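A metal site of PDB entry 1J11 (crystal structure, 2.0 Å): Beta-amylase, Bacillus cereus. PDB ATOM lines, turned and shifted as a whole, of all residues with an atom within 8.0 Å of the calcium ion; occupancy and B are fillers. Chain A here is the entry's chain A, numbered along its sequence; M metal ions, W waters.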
ATOM      1  N   TRP A  52      -9.945  28.834 -23.736  1.00  0.00           N
ATOM      2  CA  TRP A  52     -10.464  27.887 -22.750  1.00  0.00           C
ATOM      3  C   TRP A  52      -9.481  26.711 -22.681  1.00  0.00           C
ATOM      4  O   TRP A  52      -9.204  26.192 -21.589  1.00  0.00           O
ATOM      5  CB  TRP A  52     -11.865  27.409 -23.163  1.00  0.00           C
ATOM      6  CG  TRP A  52     -12.566  26.582 -22.101  1.00  0.00           C
ATOM      7  CD1 TRP A  52     -12.233  26.492 -20.774  1.00  0.00           C
ATOM      8  CD2 TRP A  52     -13.721  25.755 -22.281  1.00  0.00           C
ATOM      9  NE1 TRP A  52     -13.103  25.665 -20.128  1.00  0.00           N
ATOM     10  CE2 TRP A  52     -14.034  25.188 -21.019  1.00  0.00           C
ATOM     11  CE3 TRP A  52     -14.523  25.415 -23.384  1.00  0.00           C
ATOM     12  CZ2 TRP A  52     -15.112  24.313 -20.828  1.00  0.00           C
ATOM     13  CZ3 TRP A  52     -15.596  24.548 -23.197  1.00  0.00           C
ATOM     14  CH2 TRP A  52     -15.882  24.011 -21.921  1.00  0.00           C
ATOM     15  N   GLU A  56      -8.293  25.993 -18.523  1.00  0.00           N
ATOM     16  CA  GLU A  56      -8.847  24.848 -17.781  1.00  0.00           C
ATOM     17  C   GLU A  56      -8.466  23.600 -18.548  1.00  0.00           C
ATOM     18  O   GLU A  56      -9.279  22.716 -18.777  1.00  0.00           O
ATOM     19  CB  GLU A  56     -10.376  24.973 -17.697  1.00  0.00           C
ATOM     20  CG  GLU A  56     -11.019  24.086 -16.643  1.00  0.00           C
ATOM     21  CD  GLU A  56     -12.512  24.332 -16.498  1.00  0.00           C
ATOM     22  OE1 GLU A  56     -13.062  25.146 -17.254  1.00  0.00           O
ATOM     23  OE2 GLU A  56     -13.122  23.714 -15.618  1.00  0.00           O
ATOM     24  N   GLY A  59      -8.156  19.599 -16.378  1.00  0.00           N
ATOM     25  CA  GLY A  59      -9.356  18.999 -15.827  1.00  0.00           C
ATOM     26  C   GLY A  59     -10.307  20.023 -15.260  1.00  0.00           C
ATOM     27  O   GLY A  59      -9.988  21.202 -15.140  1.00  0.00           O
ATOM     28  N   ASP A  60     -11.492  19.539 -14.911  1.00  0.00           N
ATOM     29  CA  ASP A  60     -12.538  20.370 -14.360  1.00  0.00           C
ATOM     30  C   ASP A  60     -12.025  21.121 -13.131  1.00  0.00           C
ATOM     31  O   ASP A  60     -11.516  20.520 -12.185  1.00  0.00           O
ATOM     32  CB  ASP A  60     -13.746  19.518 -13.986  1.00  0.00           C
ATOM     33  CG  ASP A  60     -14.941  20.340 -13.594  1.00  0.00           C
ATOM     34  OD1 ASP A  60     -15.021  21.507 -14.017  1.00  0.00           O
ATOM     35  OD2 ASP A  60     -15.808  19.841 -12.851  1.00  0.00           O
ATOM     36  N   GLN A  61     -12.187  22.449 -13.182  1.00  0.00           N
ATOM     37  CA  GLN A  61     -11.779  23.369 -12.125  1.00  0.00           C
ATOM     38  C   GLN A  61     -10.277  23.480 -11.928  1.00  0.00           C
ATOM     39  O   GLN A  61      -9.810  24.052 -10.941  1.00  0.00           O
ATOM     40  CB  GLN A  61     -12.499  23.069 -10.807  1.00  0.00           C
ATOM     41  CG  GLN A  61     -14.022  23.091 -10.879  1.00  0.00           C
ATOM     42  CD  GLN A  61     -14.574  24.366 -11.469  1.00  0.00           C
ATOM     43  OE1 GLN A  61     -14.634  24.522 -12.691  1.00  0.00           O
ATOM     44  NE2 GLN A  61     -14.985  25.297 -10.625  1.00  0.00           N
ATOM     45  N   GLN A  62      -9.498  22.919 -12.848  1.00  0.00           N
ATOM     46  CA  GLN A  62      -8.053  23.017 -12.767  1.00  0.00           C
ATOM     47  C   GLN A  62      -7.651  24.213 -13.621  1.00  0.00           C
ATOM     48  O   GLN A  62      -7.083  24.080 -14.704  1.00  0.00           O
ATOM     49  CB  GLN A  62      -7.414  21.726 -13.239  1.00  0.00           C
ATOM     50  CG  GLN A  62      -7.774  20.580 -12.337  1.00  0.00           C
ATOM     51  CD  GLN A  62      -7.061  19.319 -12.717  1.00  0.00           C
ATOM     52  OE1 GLN A  62      -5.853  19.330 -12.998  1.00  0.00           O
ATOM     53  NE2 GLN A  62      -7.797  18.216 -12.750  1.00  0.00           N
ATOM     54  N   PHE A  63      -7.944  25.389 -13.085  1.00  0.00           N
ATOM     55  CA  PHE A  63      -7.713  26.664 -13.733  1.00  0.00           C
ATOM     56  C   PHE A  63      -6.275  27.184 -13.752  1.00  0.00           C
ATOM     57  O   PHE A  63      -5.494  26.940 -12.838  1.00  0.00           O
ATOM     58  CB  PHE A  63      -8.618  27.716 -13.104  1.00  0.00           C
ATOM     59  CG  PHE A  63     -10.096  27.471 -13.324  1.00  0.00           C
ATOM     60  CD1 PHE A  63     -10.960  27.356 -12.239  1.00  0.00           C
ATOM     61  CD2 PHE A  63     -10.619  27.407 -14.620  1.00  0.00           C
ATOM     62  CE1 PHE A  63     -12.339  27.187 -12.447  1.00  0.00           C
ATOM     63  CE2 PHE A  63     -11.985  27.234 -14.822  1.00  0.00           C
ATOM     64  CZ  PHE A  63     -12.845  27.127 -13.741  1.00  0.00           C
ATOM     65  N   TRP A 106     -11.023  16.918 -21.856  1.00  0.00           N
ATOM     66  CA  TRP A 106     -11.794  16.196 -20.833  1.00  0.00           C
ATOM     67  C   TRP A 106     -13.276  16.533 -20.919  1.00  0.00           C
ATOM     68  O   TRP A 106     -14.129  15.781 -20.458  1.00  0.00           O
ATOM     69  CB  TRP A 106     -11.245  16.514 -19.415  1.00  0.00           C
ATOM     70  CG  TRP A 106     -11.259  17.982 -19.064  1.00  0.00           C
ATOM     71  CD1 TRP A 106     -10.201  18.863 -19.187  1.00  0.00           C
ATOM     72  CD2 TRP A 106     -12.366  18.750 -18.582  1.00  0.00           C
ATOM     73  NE1 TRP A 106     -10.608  20.125 -18.825  1.00  0.00           N
ATOM     74  CE2 TRP A 106     -11.926  20.085 -18.443  1.00  0.00           C
ATOM     75  CE3 TRP A 106     -13.689  18.443 -18.250  1.00  0.00           C
ATOM     76  CZ2 TRP A 106     -12.766  21.114 -17.996  1.00  0.00           C
ATOM     77  CZ3 TRP A 106     -14.534  19.464 -17.799  1.00  0.00           C
ATOM     78  CH2 TRP A 106     -14.063  20.783 -17.685  1.00  0.00           C
ATOM     79  N   VAL A 107     -13.582  17.677 -21.537  1.00  0.00           N
ATOM     80  CA  VAL A 107     -14.960  18.118 -21.677  1.00  0.00           C
ATOM     81  C   VAL A 107     -15.811  17.119 -22.465  1.00  0.00           C
ATOM     82  O   VAL A 107     -16.943  16.818 -22.088  1.00  0.00           O
ATOM     83  CB  VAL A 107     -15.033  19.514 -22.332  1.00  0.00           C
ATOM     84  CG1 VAL A 107     -16.478  19.891 -22.654  1.00  0.00           C
ATOM     85  CG2 VAL A 107     -14.421  20.549 -21.398  1.00  0.00           C
ATOM     86  N   GLN A 110     -17.708  14.247 -20.761  1.00  0.00           N
ATOM     87  CA  GLN A 110     -18.817  14.580 -19.859  1.00  0.00           C
ATOM     88  C   GLN A 110     -20.146  13.950 -20.306  1.00  0.00           C
ATOM     89  O   GLN A 110     -21.094  13.849 -19.514  1.00  0.00           O
ATOM     90  CB  GLN A 110     -18.978  16.100 -19.739  1.00  0.00           C
ATOM     91  CG  GLN A 110     -17.744  16.843 -19.215  1.00  0.00           C
ATOM     92  CD  GLN A 110     -17.289  16.346 -17.855  1.00  0.00           C
ATOM     93  OE1 GLN A 110     -16.361  15.538 -17.746  1.00  0.00           O
ATOM     94  NE2 GLN A 110     -17.949  16.835 -16.801  1.00  0.00           N
ATOM     95  N   VAL A 137     -24.572  21.417 -19.882  1.00  0.00           N
ATOM     96  CA  VAL A 137     -23.115  21.432 -19.780  1.00  0.00           C
ATOM     97  C   VAL A 137     -22.622  22.886 -19.947  1.00  0.00           C
ATOM     98  O   VAL A 137     -21.687  23.308 -19.268  1.00  0.00           O
ATOM     99  CB  VAL A 137     -22.463  20.539 -20.867  1.00  0.00           C
ATOM    100  CG1 VAL A 137     -20.942  20.653 -20.820  1.00  0.00           C
ATOM    101  CG2 VAL A 137     -22.876  19.085 -20.663  1.00  0.00           C
ATOM    102  N   LYS A 140     -23.130  24.888 -16.782  1.00  0.00           N
ATOM    103  CA  LYS A 140     -22.154  24.500 -15.773  1.00  0.00           C
ATOM    104  C   LYS A 140     -20.757  25.040 -16.052  1.00  0.00           C
ATOM    105  O   LYS A 140     -20.222  25.828 -15.282  1.00  0.00           O
ATOM    106  CB  LYS A 140     -22.064  22.976 -15.646  1.00  0.00           C
ATOM    107  CG  LYS A 140     -20.970  22.542 -14.682  1.00  0.00           C
ATOM    108  CD  LYS A 140     -20.787  21.045 -14.599  1.00  0.00           C
ATOM    109  CE  LYS A 140     -19.675  20.697 -13.615  1.00  0.00           C
ATOM    110  NZ  LYS A 140     -18.315  21.040 -14.113  1.00  0.00           N
ATOM    111  N   GLU A 141     -20.187  24.606 -17.170  1.00  0.00           N
ATOM    112  CA  GLU A 141     -18.841  25.010 -17.557  1.00  0.00           C
ATOM    113  C   GLU A 141     -18.642  26.497 -17.800  1.00  0.00           C
ATOM    114  O   GLU A 141     -17.674  27.070 -17.307  1.00  0.00           O
ATOM    115  CB  GLU A 141     -18.381  24.181 -18.748  1.00  0.00           C
ATOM    116  CG  GLU A 141     -18.480  22.660 -18.517  1.00  0.00           C
ATOM    117  CD  GLU A 141     -17.617  22.136 -17.352  1.00  0.00           C
ATOM    118  OE1 GLU A 141     -16.692  22.850 -16.897  1.00  0.00           O
ATOM    119  OE2 GLU A 141     -17.842  20.990 -16.917  1.00  0.00           O
ATOM    120  N   TYR A 142     -19.534  27.146 -18.558  1.00  0.00           N
ATOM    121  CA  TYR A 142     -19.387  28.583 -18.809  1.00  0.00           C
ATOM    122  C   TYR A 142     -19.591  29.357 -17.529  1.00  0.00           C
ATOM    123  O   TYR A 142     -18.898  30.330 -17.274  1.00  0.00           O
ATOM    124  CB  TYR A 142     -20.356  29.107 -19.883  1.00  0.00           C
ATOM    125  CG  TYR A 142     -20.021  28.700 -21.306  1.00  0.00           C
ATOM    126  CD1 TYR A 142     -19.305  27.527 -21.577  1.00  0.00           C
ATOM    127  CD2 TYR A 142     -20.473  29.461 -22.395  1.00  0.00           C
ATOM    128  CE1 TYR A 142     -19.045  27.130 -22.880  1.00  0.00           C
ATOM    129  CE2 TYR A 142     -20.213  29.064 -23.698  1.00  0.00           C
ATOM    130  CZ  TYR A 142     -19.507  27.897 -23.941  1.00  0.00           C
ATOM    131  OH  TYR A 142     -19.258  27.491 -25.225  1.00  0.00           O
ATOM    132  N   GLY A 143     -20.548  28.927 -16.715  1.00  0.00           N
ATOM    133  CA  GLY A 143     -20.795  29.601 -15.460  1.00  0.00           C
ATOM    134  C   GLY A 143     -19.547  29.557 -14.586  1.00  0.00           C
ATOM    135  O   GLY A 143     -19.104  30.593 -14.067  1.00  0.00           O
ATOM    136  N   GLU A 144     -18.964  28.364 -14.480  1.00  0.00           N
ATOM    137  CA  GLU A 144     -17.771  28.142 -13.680  1.00  0.00           C
ATOM    138  C   GLU A 144     -16.569  28.918 -14.220  1.00  0.00           C
ATOM    139  O   GLU A 144     -15.819  29.525 -13.464  1.00  0.00           O
ATOM    140  CB  GLU A 144     -17.437  26.652 -13.623  1.00  0.00           C
ATOM    141  CG  GLU A 144     -18.390  25.833 -12.748  1.00  0.00           C
ATOM    142  CD  GLU A 144     -18.153  24.332 -12.845  1.00  0.00           C
ATOM    143  OE1 GLU A 144     -17.544  23.879 -13.831  1.00  0.00           O
ATOM    144  OE2 GLU A 144     -18.587  23.599 -11.934  1.00  0.00           O
ATOM    145  N   LEU A 145     -16.396  28.872 -15.531  1.00  0.00           N
ATOM    146  CA  LEU A 145     -15.303  29.578 -16.184  1.00  0.00           C
ATOM    147  C   LEU A 145     -15.438  31.106 -16.044  1.00  0.00           C
ATOM    148  O   LEU A 145     -14.481  31.777 -15.691  1.00  0.00           O
ATOM    149  CB  LEU A 145     -15.221  29.193 -17.658  1.00  0.00           C
ATOM    150  CG  LEU A 145     -14.098  29.855 -18.445  1.00  0.00           C
ATOM    151  CD1 LEU A 145     -12.732  29.389 -17.936  1.00  0.00           C
ATOM    152  CD2 LEU A 145     -14.266  29.534 -19.910  1.00  0.00           C
ATOM    153  N   ALA A 148     -14.805  32.090 -12.384  1.00  0.00           N
ATOM    154  CA  ALA A 148     -13.389  31.963 -12.036  1.00  0.00           C
ATOM    155  C   ALA A 148     -12.557  33.070 -12.703  1.00  0.00           C
ATOM    156  O   ALA A 148     -11.667  33.639 -12.074  1.00  0.00           O
ATOM    157  CB  ALA A 148     -12.875  30.594 -12.424  1.00  0.00           C
HETATM  158 CA    CA M   1     -15.447  23.672 -14.892  1.00  0.00          CA
HETATM  159  O   HOH W   1     -15.533  25.800 -16.339  1.00  0.00           O
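OE2 of Glu 144 lies within salt-bridge range of NZ of Lys 140. The side-chain carboxylate of Asp 60 is in salt-bridge range of the side-chain amino group of Lys 140 (3.1 Å). The indole nitrogen (NE1) of Trp 106 sits at hydrogen-bond distance from the backbone carbonyl oxygen (O) of Glu 56 (2.9 Å). The indole nitrogen of Trp 52 lies within hydrogen-bond range of the side-chain carboxylate of Glu 56, at 2.9 Å. The side-chain carboxylate (OE2) of Glu 141 lies within salt-bridge range of the side-chain amino group (NZ) of Lys 140 (2.8 Å).
Residues that only touch the calcium ion: Lys 140 (3.97 Å). Within 4 Å of the calcium ion: Glu 56, Asp 60, Gln 61, Lys 140, Glu 141 and Glu 144. The nearest printed residue that does not touch the calcium ion is Trp 106 (4.3 Å).
OE1 of Glu 144 is bound to the calcium ion (2.4 Å). The side-chain carboxylate (OD1) of Asp 60 is bound to the calcium ion, 2.4 Å away. The side-chain carboxylate (OE2) of Glu 56 binds the calcium ion (2.4 Å). The calcium ion is bound by the side-chain amide oxygen (OE1) of Gln 61 (2.5 Å). The calcium ion is bound by OE1 of Glu 141, 2.5 Å away. The calcium ion is bound by water W1. The calcium ion has six donor atoms within binding distance.
Water W1 lies within hydrogen-bond range of O of Glu 141 (2.7 Å), OE1 of Glu 56 (2.7 Å) and N of Leu 145 (3.3 Å).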
